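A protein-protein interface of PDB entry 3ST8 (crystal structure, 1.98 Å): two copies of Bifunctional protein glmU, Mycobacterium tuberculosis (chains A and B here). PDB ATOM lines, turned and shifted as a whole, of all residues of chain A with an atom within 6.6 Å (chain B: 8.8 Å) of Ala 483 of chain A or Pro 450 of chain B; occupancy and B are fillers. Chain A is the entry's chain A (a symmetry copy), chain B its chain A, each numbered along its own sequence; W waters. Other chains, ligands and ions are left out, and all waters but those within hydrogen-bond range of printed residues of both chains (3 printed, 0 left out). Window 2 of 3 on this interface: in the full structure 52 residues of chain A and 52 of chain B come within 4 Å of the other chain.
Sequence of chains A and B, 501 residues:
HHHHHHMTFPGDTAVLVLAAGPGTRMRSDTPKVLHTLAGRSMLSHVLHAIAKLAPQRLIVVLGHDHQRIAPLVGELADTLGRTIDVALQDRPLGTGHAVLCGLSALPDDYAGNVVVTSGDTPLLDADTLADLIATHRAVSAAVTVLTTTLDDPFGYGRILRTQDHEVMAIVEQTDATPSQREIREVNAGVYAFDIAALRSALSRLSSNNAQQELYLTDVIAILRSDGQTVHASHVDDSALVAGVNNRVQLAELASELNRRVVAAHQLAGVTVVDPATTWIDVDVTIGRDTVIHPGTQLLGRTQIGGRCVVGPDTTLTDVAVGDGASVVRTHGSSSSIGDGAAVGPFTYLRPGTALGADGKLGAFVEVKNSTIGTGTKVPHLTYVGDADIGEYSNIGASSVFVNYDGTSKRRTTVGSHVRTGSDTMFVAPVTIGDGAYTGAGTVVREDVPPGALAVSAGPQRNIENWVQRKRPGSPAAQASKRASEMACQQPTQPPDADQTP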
ATOM      1  N   GLU A 464       3.759 -11.607 -17.556  1.00  0.00           N
ATOM      2  CA  GLU A 464       3.608 -11.967 -16.141  1.00  0.00           C
ATOM      3  C   GLU A 464       4.153 -13.359 -15.872  1.00  0.00           C
ATOM      4  O   GLU A 464       4.069 -14.211 -16.758  1.00  0.00           O
ATOM      5  CB  GLU A 464       2.129 -11.849 -15.707  1.00  0.00           C
ATOM      6  CG  GLU A 464       1.862 -10.325 -15.409  1.00  0.00           C
ATOM      7  CD  GLU A 464       0.412  -9.972 -14.943  1.00  0.00           C
ATOM      8  OE1 GLU A 464       0.020 -10.365 -13.834  1.00  0.00           O
ATOM      9  OE2 GLU A 464      -0.314  -9.266 -15.681  1.00  0.00           O
ATOM     10  N   ASN A 465       4.722 -13.569 -14.701  1.00  0.00           N
ATOM     11  CA  ASN A 465       5.269 -14.876 -14.290  1.00  0.00           C
ATOM     12  C   ASN A 465       6.480 -15.300 -15.088  1.00  0.00           C
ATOM     13  O   ASN A 465       6.916 -16.509 -14.993  1.00  0.00           O
ATOM     14  CB  ASN A 465       4.207 -16.022 -14.424  1.00  0.00           C
ATOM     15  CG  ASN A 465       2.960 -15.710 -13.659  1.00  0.00           C
ATOM     16  OD1 ASN A 465       3.027 -15.421 -12.454  1.00  0.00           O
ATOM     17  ND2 ASN A 465       1.809 -15.695 -14.362  1.00  0.00           N
ATOM     18  N   VAL A 467       9.507 -14.576 -14.594  1.00  0.00           N
ATOM     19  CA  VAL A 467      10.686 -14.846 -13.758  1.00  0.00           C
ATOM     20  C   VAL A 467      10.578 -16.259 -13.100  1.00  0.00           C
ATOM     21  O   VAL A 467      11.530 -17.007 -13.023  1.00  0.00           O
ATOM     22  CB  VAL A 467      10.877 -13.759 -12.677  1.00  0.00           C
ATOM     23  CG1 VAL A 467      12.038 -14.142 -11.680  1.00  0.00           C
ATOM     24  CG2 VAL A 467      11.273 -12.366 -13.409  1.00  0.00           C
ATOM     25  N   GLN A 478      12.232 -16.278  -6.111  1.00  0.00           N
ATOM     26  CA  GLN A 478      11.834 -16.350  -4.675  1.00  0.00           C
ATOM     27  C   GLN A 478      11.260 -15.019  -4.177  1.00  0.00           C
ATOM     28  O   GLN A 478      10.228 -15.001  -3.501  1.00  0.00           O
ATOM     29  CB  GLN A 478      12.992 -16.843  -3.766  1.00  0.00           C
ATOM     30  CG  GLN A 478      13.443 -18.276  -4.145  1.00  0.00           C
ATOM     31  CD  GLN A 478      14.824 -18.735  -3.549  1.00  0.00           C
ATOM     32  OE1 GLN A 478      15.651 -17.936  -3.077  1.00  0.00           O
ATOM     33  NE2 GLN A 478      15.067 -20.056  -3.604  1.00  0.00           N
ATOM     34  N   ALA A 479      11.904 -13.880  -4.493  1.00  0.00           N
ATOM     35  CA  ALA A 479      11.315 -12.585  -4.150  1.00  0.00           C
ATOM     36  C   ALA A 479       9.981 -12.312  -4.828  1.00  0.00           C
ATOM     37  O   ALA A 479       9.079 -11.708  -4.188  1.00  0.00           O
ATOM     38  CB  ALA A 479      12.348 -11.380  -4.446  1.00  0.00           C
ATOM     39  N   SER A 480       9.753 -12.718  -6.066  1.00  0.00           N
ATOM     40  CA  SER A 480       8.414 -12.358  -6.543  1.00  0.00           C
ATOM     41  C   SER A 480       7.394 -13.298  -5.926  1.00  0.00           C
ATOM     42  O   SER A 480       6.296 -12.814  -5.637  1.00  0.00           O
ATOM     43  CB  SER A 480       8.141 -12.357  -8.012  1.00  0.00           C
ATOM     44  OG  SER A 480       8.669 -13.482  -8.562  1.00  0.00           O
ATOM     45  N   LYS A 481       7.773 -14.552  -5.668  1.00  0.00           N
ATOM     46  CA  LYS A 481       6.863 -15.492  -4.886  1.00  0.00           C
ATOM     47  C   LYS A 481       6.527 -14.847  -3.523  1.00  0.00           C
ATOM     48  O   LYS A 481       5.361 -14.752  -3.137  1.00  0.00           O
ATOM     49  CB  LYS A 481       7.531 -16.850  -4.729  1.00  0.00           C
ATOM     50  CG  LYS A 481       6.615 -18.116  -4.537  1.00  0.00           C
ATOM     51  CD  LYS A 481       7.373 -19.520  -4.848  1.00  0.00           C
ATOM     52  CE  LYS A 481       8.030 -19.699  -6.305  1.00  0.00           C
ATOM     53  NZ  LYS A 481       9.577 -19.516  -6.424  1.00  0.00           N
ATOM     54  N   ARG A 482       7.517 -14.313  -2.809  1.00  0.00           N
ATOM     55  CA  ARG A 482       7.250 -13.638  -1.497  1.00  0.00           C
ATOM     56  C   ARG A 482       6.244 -12.470  -1.636  1.00  0.00           C
ATOM     57  O   ARG A 482       5.308 -12.326  -0.823  1.00  0.00           O
ATOM     58  CB  ARG A 482       8.545 -13.167  -0.736  1.00  0.00           C
ATOM     59  CG  ARG A 482       9.453 -14.218  -0.062  1.00  0.00           C
ATOM     60  CD  ARG A 482      10.810 -13.584   0.406  1.00  0.00           C
ATOM     61  NE  ARG A 482      12.012 -13.999  -0.409  1.00  0.00           N
ATOM     62  CZ  ARG A 482      12.901 -13.174  -0.958  1.00  0.00           C
ATOM     63  NH1 ARG A 482      12.751 -11.872  -0.829  1.00  0.00           N
ATOM     64  NH2 ARG A 482      13.945 -13.641  -1.676  1.00  0.00           N
ATOM     65  N   ALA A 483       6.428 -11.636  -2.645  1.00  0.00           N
ATOM     66  CA  ALA A 483       5.572 -10.469  -2.863  1.00  0.00           C
ATOM     67  C   ALA A 483       4.180 -10.951  -3.216  1.00  0.00           C
ATOM     68  O   ALA A 483       3.231 -10.389  -2.696  1.00  0.00           O
ATOM     69  CB  ALA A 483       6.117  -9.491  -3.979  1.00  0.00           C
ATOM     70  N   SER A 484       4.051 -11.958  -4.091  1.00  0.00           N
ATOM     71  CA  SER A 484       2.727 -12.440  -4.517  1.00  0.00           C
ATOM     72  C   SER A 484       1.861 -12.923  -3.326  1.00  0.00           C
ATOM     73  O   SER A 484       0.658 -12.745  -3.356  1.00  0.00           O
ATOM     74  CB  SER A 484       2.849 -13.529  -5.569  1.00  0.00           C
ATOM     75  OG  SER A 484       2.799 -14.775  -4.892  1.00  0.00           O
ATOM     76  N   GLU A 485       2.451 -13.504  -2.273  1.00  0.00           N
ATOM     77  CA  GLU A 485       1.754 -13.596  -0.965  1.00  0.00           C
ATOM     78  C   GLU A 485       1.653 -12.264  -0.184  1.00  0.00           C
ATOM     79  O   GLU A 485       0.803 -11.402  -0.512  1.00  0.00           O
ATOM     80  CB  GLU A 485       2.412 -14.653  -0.106  1.00  0.00           C
ATOM     81  CG  GLU A 485       2.455 -15.962  -0.819  1.00  0.00           C
ATOM     82  CD  GLU A 485       3.665 -16.754  -0.437  1.00  0.00           C
ATOM     83  OE1 GLU A 485       3.954 -17.754  -1.126  1.00  0.00           O
ATOM     84  OE2 GLU A 485       4.346 -16.368   0.546  1.00  0.00           O
ATOM     85  N   MET A 486       2.500 -12.111   0.844  1.00  0.00           N
ATOM     86  CA  MET A 486       2.591 -10.870   1.634  1.00  0.00           C
ATOM     87  C   MET A 486       1.216 -10.231   1.880  1.00  0.00           C
ATOM     88  O   MET A 486       0.607  -9.642   0.967  1.00  0.00           O
ATOM     89  CB  MET A 486       3.505  -9.854   0.932  1.00  0.00           C
ATOM     90  CG  MET A 486       4.215  -8.841   1.847  1.00  0.00           C
ATOM     91  SD  MET A 486       5.768  -9.487   2.577  1.00  0.00           S
ATOM     92  CE  MET A 486       6.580  -7.921   3.102  1.00  0.00           C
ATOM     93  N   GLY B 415      11.770  -2.367  -6.704  1.00  0.00           N
ATOM     94  CA  GLY B 415      11.841  -3.323  -5.536  1.00  0.00           C
ATOM     95  C   GLY B 415      13.173  -3.975  -5.303  1.00  0.00           C
ATOM     96  O   GLY B 415      14.267  -3.546  -5.842  1.00  0.00           O
ATOM     97  N   SER B 416      13.130  -5.085  -4.552  1.00  0.00           N
ATOM     98  CA  SER B 416      14.315  -5.811  -4.221  1.00  0.00           C
ATOM     99  C   SER B 416      14.478  -6.982  -5.168  1.00  0.00           C
ATOM    100  O   SER B 416      13.462  -7.500  -5.682  1.00  0.00           O
ATOM    101  CB  SER B 416      14.140  -6.387  -2.751  1.00  0.00           C
ATOM    102  OG  SER B 416      14.187  -5.186  -1.925  1.00  0.00           O
ATOM    103  N   VAL B 418      15.574  -7.174  -8.041  1.00  0.00           N
ATOM    104  CA  VAL B 418      15.165  -7.047  -9.406  1.00  0.00           C
ATOM    105  C   VAL B 418      16.450  -7.194 -10.325  1.00  0.00           C
ATOM    106  O   VAL B 418      17.612  -7.016  -9.856  1.00  0.00           O
ATOM    107  CB  VAL B 418      14.459  -5.726  -9.717  1.00  0.00           C
ATOM    108  CG1 VAL B 418      13.333  -5.480  -8.657  1.00  0.00           C
ATOM    109  CG2 VAL B 418      15.549  -4.537  -9.806  1.00  0.00           C
ATOM    110  N   THR B 431       6.615   2.002 -10.913  1.00  0.00           N
ATOM    111  CA  THR B 431       7.089   1.122  -9.836  1.00  0.00           C
ATOM    112  C   THR B 431       7.473  -0.216 -10.458  1.00  0.00           C
ATOM    113  O   THR B 431       6.728  -0.734 -11.297  1.00  0.00           O
ATOM    114  CB  THR B 431       5.917   0.824  -8.878  1.00  0.00           C
ATOM    115  OG1 THR B 431       5.566   2.075  -8.267  1.00  0.00           O
ATOM    116  CG2 THR B 431       6.339  -0.148  -7.744  1.00  0.00           C
ATOM    117  N   ILE B 432       8.624  -0.777 -10.086  1.00  0.00           N
ATOM    118  CA  ILE B 432       9.025  -2.072 -10.621  1.00  0.00           C
ATOM    119  C   ILE B 432       8.948  -3.061  -9.448  1.00  0.00           C
ATOM    120  O   ILE B 432       9.575  -2.870  -8.403  1.00  0.00           O
ATOM    121  CB  ILE B 432      10.499  -2.068 -11.047  1.00  0.00           C
ATOM    122  CG1 ILE B 432      10.776  -0.952 -12.043  1.00  0.00           C
ATOM    123  CG2 ILE B 432      10.968  -3.462 -11.571  1.00  0.00           C
ATOM    124  CD1 ILE B 432      10.064  -0.997 -13.318  1.00  0.00           C
ATOM    125  N   GLY B 433       8.135  -4.104  -9.588  1.00  0.00           N
ATOM    126  CA  GLY B 433       7.927  -4.949  -8.380  1.00  0.00           C
ATOM    127  C   GLY B 433       9.103  -5.870  -8.041  1.00  0.00           C
ATOM    128  O   GLY B 433      10.040  -6.096  -8.879  1.00  0.00           O
ATOM    129  N   ASP B 434       9.072  -6.476  -6.855  1.00  0.00           N
ATOM    130  CA  ASP B 434      10.188  -7.325  -6.442  1.00  0.00           C
ATOM    131  C   ASP B 434      10.417  -8.442  -7.466  1.00  0.00           C
ATOM    132  O   ASP B 434       9.468  -9.004  -7.962  1.00  0.00           O
ATOM    133  CB  ASP B 434       9.967  -7.984  -5.053  1.00  0.00           C
ATOM    134  CG  ASP B 434       9.909  -6.955  -3.923  1.00  0.00           C
ATOM    135  OD1 ASP B 434      10.404  -5.767  -4.045  1.00  0.00           O
ATOM    136  OD2 ASP B 434       9.409  -7.380  -2.861  1.00  0.00           O
ATOM    137  N   GLY B 435      11.698  -8.744  -7.712  1.00  0.00           N
ATOM    138  CA  GLY B 435      12.126  -9.907  -8.505  1.00  0.00           C
ATOM    139  C   GLY B 435      11.767  -9.710  -9.993  1.00  0.00           C
ATOM    140  O   GLY B 435      11.930 -10.680 -10.763  1.00  0.00           O
ATOM    141  N   ALA B 436      11.256  -8.523 -10.416  1.00  0.00           N
ATOM    142  CA  ALA B 436      10.969  -8.297 -11.850  1.00  0.00           C
ATOM    143  C   ALA B 436      12.239  -8.149 -12.721  1.00  0.00           C
ATOM    144  O   ALA B 436      13.285  -7.827 -12.229  1.00  0.00           O
ATOM    145  CB  ALA B 436      10.095  -7.042 -12.104  1.00  0.00           C
ATOM    146  N   TYR B 437      12.116  -8.353 -14.023  1.00  0.00           N
ATOM    147  CA  TYR B 437      13.268  -8.156 -14.951  1.00  0.00           C
ATOM    148  C   TYR B 437      12.763  -7.117 -15.945  1.00  0.00           C
ATOM    149  O   TYR B 437      11.536  -7.010 -16.163  1.00  0.00           O
ATOM    150  CB  TYR B 437      13.510  -9.403 -15.794  1.00  0.00           C
ATOM    151  CG  TYR B 437      14.551 -10.342 -15.230  1.00  0.00           C
ATOM    152  CD1 TYR B 437      15.590 -10.758 -16.049  1.00  0.00           C
ATOM    153  CD2 TYR B 437      14.408 -10.909 -13.904  1.00  0.00           C
ATOM    154  CE1 TYR B 437      16.578 -11.695 -15.564  1.00  0.00           C
ATOM    155  CE2 TYR B 437      15.403 -11.858 -13.417  1.00  0.00           C
ATOM    156  CZ  TYR B 437      16.470 -12.221 -14.271  1.00  0.00           C
ATOM    157  OH  TYR B 437      17.443 -13.153 -13.884  1.00  0.00           O
ATOM    158  N   ASP B 447       3.780   0.526 -14.524  1.00  0.00           N
ATOM    159  CA  ASP B 447       4.302  -0.385 -13.510  1.00  0.00           C
ATOM    160  C   ASP B 447       4.563  -1.781 -14.036  1.00  0.00           C
ATOM    161  O   ASP B 447       3.875  -2.276 -14.974  1.00  0.00           O
ATOM    162  CB  ASP B 447       3.339  -0.517 -12.316  1.00  0.00           C
ATOM    163  CG  ASP B 447       3.158   0.865 -11.565  1.00  0.00           C
ATOM    164  OD1 ASP B 447       3.943   1.842 -11.836  1.00  0.00           O
ATOM    165  OD2 ASP B 447       2.244   0.915 -10.699  1.00  0.00           O
ATOM    166  N   VAL B 448       5.521  -2.430 -13.388  1.00  0.00           N
ATOM    167  CA  VAL B 448       5.844  -3.789 -13.777  1.00  0.00           C
ATOM    168  C   VAL B 448       5.582  -4.605 -12.533  1.00  0.00           C
ATOM    169  O   VAL B 448       6.227  -4.371 -11.488  1.00  0.00           O
ATOM    170  CB  VAL B 448       7.335  -3.900 -14.130  1.00  0.00           C
ATOM    171  CG1 VAL B 448       7.717  -5.403 -14.445  1.00  0.00           C
ATOM    172  CG2 VAL B 448       7.657  -3.058 -15.346  1.00  0.00           C
ATOM    173  N   PRO B 449       4.673  -5.603 -12.611  1.00  0.00           N
ATOM    174  CA  PRO B 449       4.387  -6.429 -11.411  1.00  0.00           C
ATOM    175  C   PRO B 449       5.609  -7.245 -10.944  1.00  0.00           C
ATOM    176  O   PRO B 449       6.469  -7.555 -11.747  1.00  0.00           O
ATOM    177  CB  PRO B 449       3.241  -7.404 -11.873  1.00  0.00           C
ATOM    178  CG  PRO B 449       2.699  -6.781 -13.172  1.00  0.00           C
ATOM    179  CD  PRO B 449       3.842  -5.932 -13.777  1.00  0.00           C
ATOM    180  N   PRO B 450       5.664  -7.625  -9.661  1.00  0.00           N
ATOM    181  CA  PRO B 450       6.629  -8.574  -9.162  1.00  0.00           C
ATOM    182  C   PRO B 450       6.778  -9.795 -10.098  1.00  0.00           C
ATOM    183  O   PRO B 450       5.818 -10.326 -10.576  1.00  0.00           O
ATOM    184  CB  PRO B 450       6.039  -8.992  -7.762  1.00  0.00           C
ATOM    185  CG  PRO B 450       5.244  -7.726  -7.356  1.00  0.00           C
ATOM    186  CD  PRO B 450       4.598  -7.323  -8.652  1.00  0.00           C
ATOM    187  N   GLY B 451       8.019 -10.166 -10.440  1.00  0.00           N
ATOM    188  CA  GLY B 451       8.214 -11.419 -11.179  1.00  0.00           C
ATOM    189  C   GLY B 451       7.828 -11.338 -12.630  1.00  0.00           C
ATOM    190  O   GLY B 451       7.903 -12.379 -13.327  1.00  0.00           O
ATOM    191  N   ALA B 452       7.480 -10.151 -13.137  1.00  0.00           N
ATOM    192  CA  ALA B 452       7.152 -10.041 -14.558  1.00  0.00           C
ATOM    193  C   ALA B 452       8.444  -9.692 -15.352  1.00  0.00           C
ATOM    194  O   ALA B 452       9.402  -9.209 -14.742  1.00  0.00           O
ATOM    195  CB  ALA B 452       6.093  -8.960 -14.779  1.00  0.00           C
ATOM    196  N   LEU B 453       8.459  -9.915 -16.660  1.00  0.00           N
ATOM    197  CA  LEU B 453       9.507  -9.347 -17.533  1.00  0.00           C
ATOM    198  C   LEU B 453       8.872  -8.228 -18.341  1.00  0.00           C
ATOM    199  O   LEU B 453       7.842  -8.465 -19.035  1.00  0.00           O
ATOM    200  CB  LEU B 453      10.044 -10.416 -18.512  1.00  0.00           C
ATOM    201  CG  LEU B 453      10.852  -9.892 -19.759  1.00  0.00           C
ATOM    202  CD1 LEU B 453      12.166  -9.327 -19.291  1.00  0.00           C
ATOM    203  CD2 LEU B 453      11.185 -11.077 -20.670  1.00  0.00           C
HETATM  204  O   HOH W   1       9.443  -9.889  -2.325  1.00  0.00           O
HETATM  205  O   HOH W   2       4.393 -11.444 -12.906  1.00  0.00           O
HETATM  206  O   HOH W   3       7.447 -14.738 -11.889  1.00  0.00           O
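The backbone carbonyl oxygen of Gly 451 of chain B sits at hydrogen-bond distance from the backbone NH of Val 467 of chain A, 3.0 Å away.
N of Gly 451 of chain B sits at hydrogen-bond distance from O of Asp 434 of chain B, at 3.1 Å.
O of Ser 416 of chain B sits at hydrogen-bond distance from N of Gly 435 of chain B, 3.0 Å away.
The backbone NH of Tyr 437 of chain B lies within hydrogen-bond range of the backbone carbonyl oxygen of Ala 452 of chain B (2.9 Å).
The side-chain carboxylate of Asp 434 of chain B sits at hydrogen-bond distance from the backbone NH of Ser 416 of chain B, 2.9 Å away.
Among the printed residues, pairs that only touch across the chains: Val 467 of chain A with Gly 435 of chain B, Ser 480 of chain A with Gly 451 of chain B, Val 467 of chain A with Tyr 437 of chain B, Ser 480 of chain A with Pro 450 of chain B, Ser 480 of chain A with Asp 434 of chain B, Asn 465 of chain A with Gly 451 of chain B, Ala 483 of chain A with Pro 450 of chain B, Val 467 of chain A with Ala 452 of chain B and Ala 479 of chain A with Asp 434 of chain B.
Pro 450 of chain B touches just these residues of chain A: Ser 480 and Ala 483.
No residue of chain B comes within 4 Å of Ser 484 of chain A.
Of the printed residues of chain A, Tyr 437 of chain B touches Val 467.
Printed residues of chain A within 4 Å of Asp 434 of chain B: Ala 479 and Ser 480.
Printed residues of chain B within 4 Å of Val 467 of chain A: Gly 435 (3.2 Å), Tyr 437 (3.5 Å), Gly 451 (3.0 Å) and Ala 452 (3.9 Å).
Of the printed residues of chain A, Gly 435 of chain B touches Val 467.
Printed residues of chain A within 4 Å of Ala 452 of chain B: Val 467.
The nearest residue of chain B that does not touch Ala 483 of chain A is Asp 434 of chain B (4.1 Å).
The nearest residue of chain A that does not touch Pro 450 of chain B is Ser 484 of chain A (5.1 Å).
The nearest printed residue of chain A that does not touch Tyr 437 of chain B is Ser 480 of chain A (8.2 Å).
Among the printed residues, no Asp or Glu carboxylate lies within 4 Å of a Lys or Arg side-chain nitrogen of the other chain.
No position is printed for both chains.
Water W1 lies within hydrogen-bond range of the side-chain carboxylate of Asp 434 of chain B (2.6 Å), the backbone carbonyl oxygen of Ala 479 of chain A (2.6 Å) and the backbone NH of Ala 483 of chain A (3.5 Å).
Water W3 bridges the backbone carbonyl oxygen (O) of Gly 451 of chain B and the backbone NH (N) of Val 467 of chain A.
Water W2 lies within hydrogen-bond range of N of Asn 465 of chain A (2.8 Å), O of Pro 450 of chain B (3.0 Å) and N of Ala 452 of chain B (3.4 Å).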
